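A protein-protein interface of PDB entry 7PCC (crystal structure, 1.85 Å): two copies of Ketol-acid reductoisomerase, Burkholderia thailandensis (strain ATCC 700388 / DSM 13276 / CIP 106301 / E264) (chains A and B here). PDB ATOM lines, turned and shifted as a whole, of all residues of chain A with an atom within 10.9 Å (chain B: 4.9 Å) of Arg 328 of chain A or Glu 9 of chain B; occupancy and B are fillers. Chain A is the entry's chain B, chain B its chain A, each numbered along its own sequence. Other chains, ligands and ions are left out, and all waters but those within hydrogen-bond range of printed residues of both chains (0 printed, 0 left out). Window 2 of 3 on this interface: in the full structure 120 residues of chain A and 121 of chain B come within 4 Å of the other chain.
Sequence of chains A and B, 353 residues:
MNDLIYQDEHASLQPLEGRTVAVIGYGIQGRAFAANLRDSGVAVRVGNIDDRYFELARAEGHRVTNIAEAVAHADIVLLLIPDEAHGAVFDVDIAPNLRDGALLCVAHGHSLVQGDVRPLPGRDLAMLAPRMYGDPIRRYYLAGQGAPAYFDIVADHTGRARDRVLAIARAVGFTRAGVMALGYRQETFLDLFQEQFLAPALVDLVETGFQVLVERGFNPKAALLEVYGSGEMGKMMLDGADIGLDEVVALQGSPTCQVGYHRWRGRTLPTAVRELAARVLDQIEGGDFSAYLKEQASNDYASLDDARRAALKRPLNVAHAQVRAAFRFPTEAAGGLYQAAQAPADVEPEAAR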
ATOM      1  N   LYS A 221      15.129  -5.739  11.244  1.00  0.00           N
ATOM      2  CA  LYS A 221      15.429  -6.619  10.083  1.00  0.00           C
ATOM      3  C   LYS A 221      15.310  -8.082  10.526  1.00  0.00           C
ATOM      4  O   LYS A 221      14.660  -8.860   9.809  1.00  0.00           O
ATOM      5  CB  LYS A 221      16.814  -6.320   9.500  1.00  0.00           C
ATOM      6  CG  LYS A 221      16.900  -5.073   8.632  1.00  0.00           C
ATOM      7  CD  LYS A 221      18.172  -5.013   7.805  1.00  0.00           C
ATOM      8  CE  LYS A 221      18.389  -3.677   7.128  1.00  0.00           C
ATOM      9  NZ  LYS A 221      18.766  -2.624   8.099  1.00  0.00           N
ATOM     10  N   LEU A 225      12.623 -10.965   9.321  1.00  0.00           N
ATOM     11  CA  LEU A 225      13.124 -12.242   8.737  1.00  0.00           C
ATOM     12  C   LEU A 225      12.465 -13.437   9.436  1.00  0.00           C
ATOM     13  O   LEU A 225      11.986 -14.351   8.723  1.00  0.00           O
ATOM     14  CB  LEU A 225      14.647 -12.311   8.868  1.00  0.00           C
ATOM     15  CG  LEU A 225      15.436 -11.442   7.887  1.00  0.00           C
ATOM     16  CD1 LEU A 225      16.901 -11.385   8.285  1.00  0.00           C
ATOM     17  CD2 LEU A 225      15.289 -11.943   6.455  1.00  0.00           C
ATOM     18  N   GLY A 229      10.012 -13.049   6.597  1.00  0.00           N
ATOM     19  CA  GLY A 229      10.938 -12.482   5.596  1.00  0.00           C
ATOM     20  C   GLY A 229      12.022 -13.452   5.148  1.00  0.00           C
ATOM     21  O   GLY A 229      12.466 -13.334   3.993  1.00  0.00           O
ATOM     22  N   SER A 230      12.441 -14.376   6.021  1.00  0.00           N
ATOM     23  CA  SER A 230      13.451 -15.427   5.728  1.00  0.00           C
ATOM     24  C   SER A 230      12.876 -16.459   4.749  1.00  0.00           C
ATOM     25  O   SER A 230      13.673 -17.164   4.103  1.00  0.00           O
ATOM     26  CB  SER A 230      13.918 -16.097   6.992  1.00  0.00           C
ATOM     27  OG  SER A 230      12.892 -16.923   7.529  1.00  0.00           O
ATOM     28  N   GLY A 231      11.542 -16.566   4.680  1.00  0.00           N
ATOM     29  CA  GLY A 231      10.820 -17.594   3.905  1.00  0.00           C
ATOM     30  C   GLY A 231      10.578 -18.856   4.718  1.00  0.00           C
ATOM     31  O   GLY A 231       9.945 -19.782   4.189  1.00  0.00           O
ATOM     32  N   HIS A 320       9.951  -4.655   5.630  1.00  0.00           N
ATOM     33  CA  HIS A 320      10.062  -5.595   4.482  1.00  0.00           C
ATOM     34  C   HIS A 320      11.000  -5.014   3.418  1.00  0.00           C
ATOM     35  O   HIS A 320      11.922  -5.742   2.974  1.00  0.00           O
ATOM     36  CB  HIS A 320       8.701  -5.918   3.857  1.00  0.00           C
ATOM     37  CG  HIS A 320       8.847  -6.819   2.681  1.00  0.00           C
ATOM     38  ND1 HIS A 320       8.885  -8.193   2.807  1.00  0.00           N
ATOM     39  CD2 HIS A 320       9.048  -6.550   1.373  1.00  0.00           C
ATOM     40  CE1 HIS A 320       9.069  -8.732   1.620  1.00  0.00           C
ATOM     41  NE2 HIS A 320       9.168  -7.748   0.725  1.00  0.00           N
ATOM     42  N   ALA A 321      10.758  -3.766   3.008  1.00  0.00           N
ATOM     43  CA  ALA A 321      11.537  -3.056   1.967  1.00  0.00           C
ATOM     44  C   ALA A 321      13.004  -2.962   2.401  1.00  0.00           C
ATOM     45  O   ALA A 321      13.892  -3.194   1.552  1.00  0.00           O
ATOM     46  CB  ALA A 321      10.947  -1.691   1.702  1.00  0.00           C
ATOM     47  N   GLN A 322      13.249  -2.642   3.674  1.00  0.00           N
ATOM     48  CA  GLN A 322      14.620  -2.527   4.237  1.00  0.00           C
ATOM     49  C   GLN A 322      15.295  -3.902   4.171  1.00  0.00           C
ATOM     50  O   GLN A 322      16.467  -3.962   3.751  1.00  0.00           O
ATOM     51  CB  GLN A 322      14.578  -1.966   5.658  1.00  0.00           C
ATOM     52  CG  GLN A 322      14.236  -0.484   5.696  1.00  0.00           C
ATOM     53  CD  GLN A 322      13.824  -0.003   7.064  1.00  0.00           C
ATOM     54  OE1 GLN A 322      13.637  -0.784   7.996  1.00  0.00           O
ATOM     55  NE2 GLN A 322      13.670   1.304   7.193  1.00  0.00           N
ATOM     56  N   VAL A 323      14.574  -4.966   4.534  1.00  0.00           N
ATOM     57  CA  VAL A 323      15.110  -6.361   4.524  1.00  0.00           C
ATOM     58  C   VAL A 323      15.421  -6.773   3.080  1.00  0.00           C
ATOM     59  O   VAL A 323      16.491  -7.369   2.869  1.00  0.00           O
ATOM     60  CB  VAL A 323      14.153  -7.356   5.208  1.00  0.00           C
ATOM     61  CG1 VAL A 323      14.481  -8.799   4.851  1.00  0.00           C
ATOM     62  CG2 VAL A 323      14.155  -7.172   6.715  1.00  0.00           C
ATOM     63  N   ARG A 324      14.526  -6.469   2.134  1.00  0.00           N
ATOM     64  CA  ARG A 324      14.620  -6.951   0.726  1.00  0.00           C
ATOM     65  C   ARG A 324      15.741  -6.216  -0.021  1.00  0.00           C
ATOM     66  O   ARG A 324      16.277  -6.798  -0.981  1.00  0.00           O
ATOM     67  CB  ARG A 324      13.281  -6.815  -0.007  1.00  0.00           C
ATOM     68  CG  ARG A 324      12.414  -8.067   0.039  1.00  0.00           C
ATOM     69  CD  ARG A 324      12.973  -9.255  -0.740  1.00  0.00           C
ATOM     70  NE  ARG A 324      14.096  -9.907  -0.081  1.00  0.00           N
ATOM     71  CZ  ARG A 324      14.019 -10.672   1.010  1.00  0.00           C
ATOM     72  NH1 ARG A 324      12.859 -10.904   1.606  1.00  0.00           N
ATOM     73  NH2 ARG A 324      15.124 -11.195   1.512  1.00  0.00           N
ATOM     74  N   ALA A 325      16.085  -4.997   0.401  1.00  0.00           N
ATOM     75  CA  ALA A 325      17.194  -4.199  -0.175  1.00  0.00           C
ATOM     76  C   ALA A 325      18.544  -4.770   0.274  1.00  0.00           C
ATOM     77  O   ALA A 325      19.541  -4.560  -0.450  1.00  0.00           O
ATOM     78  CB  ALA A 325      17.055  -2.752   0.233  1.00  0.00           C
ATOM     79  N   ALA A 326      18.570  -5.450   1.426  1.00  0.00           N
ATOM     80  CA  ALA A 326      19.799  -5.857   2.151  1.00  0.00           C
ATOM     81  C   ALA A 326      20.063  -7.365   2.022  1.00  0.00           C
ATOM     82  O   ALA A 326      21.245  -7.761   2.104  1.00  0.00           O
ATOM     83  CB  ALA A 326      19.672  -5.447   3.594  1.00  0.00           C
ATOM     84  N   PHE A 327      19.013  -8.179   1.856  1.00  0.00           N
ATOM     85  CA  PHE A 327      19.097  -9.658   1.738  1.00  0.00           C
ATOM     86  C   PHE A 327      18.545 -10.091   0.379  1.00  0.00           C
ATOM     87  O   PHE A 327      17.404  -9.729   0.061  1.00  0.00           O
ATOM     88  CB  PHE A 327      18.309 -10.345   2.854  1.00  0.00           C
ATOM     89  CG  PHE A 327      18.884 -10.172   4.235  1.00  0.00           C
ATOM     90  CD1 PHE A 327      19.750 -11.114   4.764  1.00  0.00           C
ATOM     91  CD2 PHE A 327      18.546  -9.075   5.009  1.00  0.00           C
ATOM     92  CE1 PHE A 327      20.267 -10.959   6.040  1.00  0.00           C
ATOM     93  CE2 PHE A 327      19.069  -8.919   6.284  1.00  0.00           C
ATOM     94  CZ  PHE A 327      19.927  -9.862   6.797  1.00  0.00           C
ATOM     95  N   ARG A 328      19.333 -10.849  -0.386  1.00  0.00           N
ATOM     96  CA  ARG A 328      18.911 -11.416  -1.693  1.00  0.00           C
ATOM     97  C   ARG A 328      18.019 -12.628  -1.399  1.00  0.00           C
ATOM     98  O   ARG A 328      18.392 -13.446  -0.535  1.00  0.00           O
ATOM     99  CB  ARG A 328      20.145 -11.727  -2.550  1.00  0.00           C
ATOM    100  CG  ARG A 328      20.914 -10.483  -2.981  1.00  0.00           C
ATOM    101  CD  ARG A 328      22.344 -10.728  -3.442  1.00  0.00           C
ATOM    102  NE  ARG A 328      23.079  -9.471  -3.592  1.00  0.00           N
ATOM    103  CZ  ARG A 328      24.402  -9.356  -3.740  1.00  0.00           C
ATOM    104  NH1 ARG A 328      25.180 -10.426  -3.768  1.00  0.00           N
ATOM    105  NH2 ARG A 328      24.949  -8.157  -3.858  1.00  0.00           N
ATOM    106  N   PHE A 329      16.857 -12.711  -2.048  1.00  0.00           N
ATOM    107  CA  PHE A 329      15.869 -13.799  -1.832  1.00  0.00           C
ATOM    108  C   PHE A 329      15.921 -14.783  -2.997  1.00  0.00           C
ATOM    109  O   PHE A 329      15.984 -14.370  -4.150  1.00  0.00           O
ATOM    110  CB  PHE A 329      14.460 -13.233  -1.656  1.00  0.00           C
ATOM    111  CG  PHE A 329      13.500 -14.232  -1.068  1.00  0.00           C
ATOM    112  CD1 PHE A 329      12.655 -14.970  -1.883  1.00  0.00           C
ATOM    113  CD2 PHE A 329      13.491 -14.483   0.295  1.00  0.00           C
ATOM    114  CE1 PHE A 329      11.793 -15.912  -1.342  1.00  0.00           C
ATOM    115  CE2 PHE A 329      12.626 -15.423   0.834  1.00  0.00           C
ATOM    116  CZ  PHE A 329      11.779 -16.134   0.016  1.00  0.00           C
ATOM    117  N   PRO A 330      15.888 -16.111  -2.738  1.00  0.00           N
ATOM    118  CA  PRO A 330      15.810 -17.106  -3.807  1.00  0.00           C
ATOM    119  C   PRO A 330      14.482 -17.012  -4.574  1.00  0.00           C
ATOM    120  O   PRO A 330      13.450 -17.234  -3.981  1.00  0.00           O
ATOM    121  CB  PRO A 330      15.900 -18.467  -3.090  1.00  0.00           C
ATOM    122  CG  PRO A 330      16.372 -18.151  -1.685  1.00  0.00           C
ATOM    123  CD  PRO A 330      15.935 -16.729  -1.406  1.00  0.00           C
ATOM    124  N   THR A 331      14.541 -16.666  -5.860  1.00  0.00           N
ATOM    125  CA  THR A 331      13.373 -16.627  -6.780  1.00  0.00           C
ATOM    126  C   THR A 331      13.765 -17.259  -8.121  1.00  0.00           C
ATOM    127  O   THR A 331      14.941 -17.147  -8.507  1.00  0.00           O
ATOM    128  CB  THR A 331      12.863 -15.192  -6.957  1.00  0.00           C
ATOM    129  OG1 THR A 331      13.946 -14.396  -7.436  1.00  0.00           O
ATOM    130  CG2 THR A 331      12.340 -14.584  -5.677  1.00  0.00           C
ATOM    131  N   GLU A 332      12.810 -17.916  -8.785  1.00  0.00           N
ATOM    132  CA  GLU A 332      12.931 -18.383 -10.192  1.00  0.00           C
ATOM    133  C   GLU A 332      12.661 -17.195 -11.122  1.00  0.00           C
ATOM    134  O   GLU A 332      11.774 -16.379 -10.790  1.00  0.00           O
ATOM    135  CB  GLU A 332      11.940 -19.514 -10.484  1.00  0.00           C
ATOM    136  CG  GLU A 332      12.407 -20.880 -10.018  1.00  0.00           C
ATOM    137  CD  GLU A 332      11.485 -22.018 -10.426  1.00  0.00           C
ATOM    138  OE1 GLU A 332      11.994 -23.042 -10.924  1.00  0.00           O
ATOM    139  OE2 GLU A 332      10.257 -21.875 -10.247  1.00  0.00           O
ATOM    140  N   GLN B   7      27.607 -10.555   2.083  1.00  0.00           N
ATOM    141  CA  GLN B   7      27.196 -11.330   0.883  1.00  0.00           C
ATOM    142  C   GLN B   7      28.474 -11.876   0.235  1.00  0.00           C
ATOM    143  O   GLN B   7      29.541 -11.746   0.869  1.00  0.00           O
ATOM    144  CB  GLN B   7      26.315 -10.451  -0.007  1.00  0.00           C
ATOM    145  CG  GLN B   7      24.925 -10.251   0.585  1.00  0.00           C
ATOM    146  CD  GLN B   7      24.101  -9.178  -0.085  1.00  0.00           C
ATOM    147  OE1 GLN B   7      24.622  -8.225  -0.655  1.00  0.00           O
ATOM    148  NE2 GLN B   7      22.789  -9.311   0.012  1.00  0.00           N
ATOM    149  N   ASP B   8      28.370 -12.492  -0.947  1.00  0.00           N
ATOM    150  CA  ASP B   8      29.475 -13.252  -1.604  1.00  0.00           C
ATOM    151  C   ASP B   8      30.725 -12.375  -1.743  1.00  0.00           C
ATOM    152  O   ASP B   8      31.841 -12.913  -1.596  1.00  0.00           O
ATOM    153  CB  ASP B   8      29.041 -13.806  -2.963  1.00  0.00           C
ATOM    154  CG  ASP B   8      28.234 -15.087  -2.854  1.00  0.00           C
ATOM    155  OD1 ASP B   8      28.371 -15.778  -1.823  1.00  0.00           O
ATOM    156  OD2 ASP B   8      27.472 -15.381  -3.797  1.00  0.00           O
ATOM    157  N   GLU B   9      30.539 -11.081  -2.008  1.00  0.00           N
ATOM    158  CA  GLU B   9      31.623 -10.093  -2.259  1.00  0.00           C
ATOM    159  C   GLU B   9      32.392  -9.792  -0.962  1.00  0.00           C
ATOM    160  O   GLU B   9      33.477  -9.190  -1.053  1.00  0.00           O
ATOM    161  CB  GLU B   9      31.008  -8.821  -2.848  1.00  0.00           C
ATOM    162  CG  GLU B   9      30.176  -8.037  -1.845  1.00  0.00           C
ATOM    163  CD  GLU B   9      28.851  -7.514  -2.368  1.00  0.00           C
ATOM    164  OE1 GLU B   9      27.985  -8.348  -2.702  1.00  0.00           O
ATOM    165  OE2 GLU B   9      28.686  -6.276  -2.431  1.00  0.00           O
ATOM    166  N   HIS B  10      31.850 -10.184   0.197  1.00  0.00           N
ATOM    167  CA  HIS B  10      32.376  -9.846   1.547  1.00  0.00           C
ATOM    168  C   HIS B  10      32.996 -11.075   2.227  1.00  0.00           C
ATOM    169  O   HIS B  10      33.332 -10.974   3.417  1.00  0.00           O
ATOM    170  CB  HIS B  10      31.257  -9.255   2.415  1.00  0.00           C
ATOM    171  CG  HIS B  10      30.574  -8.072   1.816  1.00  0.00           C
ATOM    172  ND1 HIS B  10      29.234  -8.084   1.479  1.00  0.00           N
ATOM    173  CD2 HIS B  10      31.026  -6.836   1.514  1.00  0.00           C
ATOM    174  CE1 HIS B  10      28.892  -6.912   0.987  1.00  0.00           C
ATOM    175  NE2 HIS B  10      29.974  -6.131   0.997  1.00  0.00           N
ATOM    176  N   ALA B  11      33.130 -12.197   1.521  1.00  0.00           N
ATOM    177  CA  ALA B  11      33.616 -13.476   2.091  1.00  0.00           C
ATOM    178  C   ALA B  11      34.367 -14.259   1.017  1.00  0.00           C
ATOM    179  O   ALA B  11      34.089 -14.030  -0.165  1.00  0.00           O
ATOM    180  CB  ALA B  11      32.458 -14.271   2.646  1.00  0.00           C
ATOM    181  N   ARG B 170      29.995 -18.811   3.489  1.00  0.00           N
ATOM    182  CA  ARG B 170      30.066 -18.755   2.004  1.00  0.00           C
ATOM    183  C   ARG B 170      29.995 -20.170   1.422  1.00  0.00           C
ATOM    184  O   ARG B 170      29.220 -20.364   0.472  1.00  0.00           O
ATOM    185  CB  ARG B 170      31.329 -18.059   1.495  1.00  0.00           C
ATOM    186  CG  ARG B 170      31.425 -18.081  -0.023  1.00  0.00           C
ATOM    187  CD  ARG B 170      32.348 -17.040  -0.609  1.00  0.00           C
ATOM    188  NE  ARG B 170      32.433 -17.229  -2.050  1.00  0.00           N
ATOM    189  CZ  ARG B 170      32.769 -16.296  -2.932  1.00  0.00           C
ATOM    190  NH1 ARG B 170      33.055 -15.065  -2.542  1.00  0.00           N
ATOM    191  NH2 ARG B 170      32.808 -16.601  -4.215  1.00  0.00           N
ATOM    192  N   ARG B 176      24.929 -15.920  -0.101  1.00  0.00           N
ATOM    193  CA  ARG B 176      24.162 -15.667  -1.353  1.00  0.00           C
ATOM    194  C   ARG B 176      22.863 -14.932  -1.018  1.00  0.00           C
ATOM    195  O   ARG B 176      22.327 -14.248  -1.907  1.00  0.00           O
ATOM    196  CB  ARG B 176      23.873 -16.977  -2.084  1.00  0.00           C
ATOM    197  CG  ARG B 176      25.132 -17.733  -2.470  1.00  0.00           C
ATOM    198  CD  ARG B 176      24.779 -19.098  -2.993  1.00  0.00           C
ATOM    199  NE  ARG B 176      25.956 -19.870  -3.352  1.00  0.00           N
ATOM    200  CZ  ARG B 176      25.937 -21.149  -3.699  1.00  0.00           C
ATOM    201  NH1 ARG B 176      24.792 -21.810  -3.736  1.00  0.00           N
ATOM    202  NH2 ARG B 176      27.067 -21.762  -4.003  1.00  0.00           N
ATOM    203  N   ALA B 177      22.380 -15.075   0.217  1.00  0.00           N
ATOM    204  CA  ALA B 177      21.227 -14.329   0.765  1.00  0.00           C
ATOM    205  C   ALA B 177      21.753 -13.138   1.570  1.00  0.00           C
ATOM    206  O   ALA B 177      21.461 -11.982   1.204  1.00  0.00           O
ATOM    207  CB  ALA B 177      20.376 -15.245   1.610  1.00  0.00           C
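ND1 of His 10 of chain B sits at hydrogen-bond distance from N of Gln 7 of chain B (3.0 Å). The side-chain amide nitrogen (NE2) of Gln 7 of chain B lies within hydrogen-bond range of the backbone carbonyl oxygen (O) of Ala 177 of chain B, at 3.2 Å. The guanidinium group (NH2) of Arg 324 of chain A is in hydrogen-bond range of the backbone carbonyl oxygen (O) of Phe 327 of chain A (3.1 Å).
Among the printed residues, pairs that only touch across the chains: Phe 327 of chain A with Ala 177 of chain B (3.4 Å) and Arg 328 of chain A with Arg 176 of chain B (3.4 Å).
Lys 221 of chain A touches none of the printed residues of chain B. Gly 231 of chain A touches none of the printed residues of chain B. Printed residues of chain B within 4 Å of Ala 326 of chain A: Gln 7. Arg 328 of chain A touches just these residues of chain B: Gln 7, Glu 9, Arg 176 and Ala 177. Of chain A, only Arg 328 comes within 4 Å of Glu 9 of chain B. No residue of chain A comes within 4 Å of His 10 of chain B. Ala 11 of chain B touches none of the printed residues of chain A. Printed residues of chain A within 4 Å of Arg 176 of chain B: Arg 328. Ala 177 of chain B touches two residues of chain A. The nearest printed residue of chain B that does not touch Ala 326 of chain A is Ala 177 of chain B (4.3 Å).
The side-chain amide oxygen of Gln 7 of chain B is in hydrogen-bond range of the guanidinium group of Arg 328 of chain A (3.2 Å). The backbone carbonyl oxygen (O) of Ala 177 of chain B sits at hydrogen-bond distance from the backbone NH (N) of Arg 328 of chain A (2.9 Å). NH2 of Arg 328 of chain A is in salt-bridge range of OE1 of Glu 9 of chain B, at 3.3 Å. The side-chain amide nitrogen of Gln 7 of chain B lies within hydrogen-bond range of the backbone carbonyl oxygen of Ala 326 of chain A (3.0 Å).
No position is printed for both chains.
Of the 8 printed residues of chain B, 4 touch a printed residue of chain A. Printed residues of chain B that touch a printed residue of chain A: Gln 7, Glu 9, Arg 176 and Ala 177. Along chain A the printed residues that touch a printed residue of chain B span positions 326 to 328. Among the printed residues, 6 pairs touch across the chains. Among the printed residues, Asp or Glu carboxylates within 4 Å of a Lys or Arg side-chain nitrogen of the other chain: Arg 328 of chain A with Glu 9 of chain B (3.3 Å).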
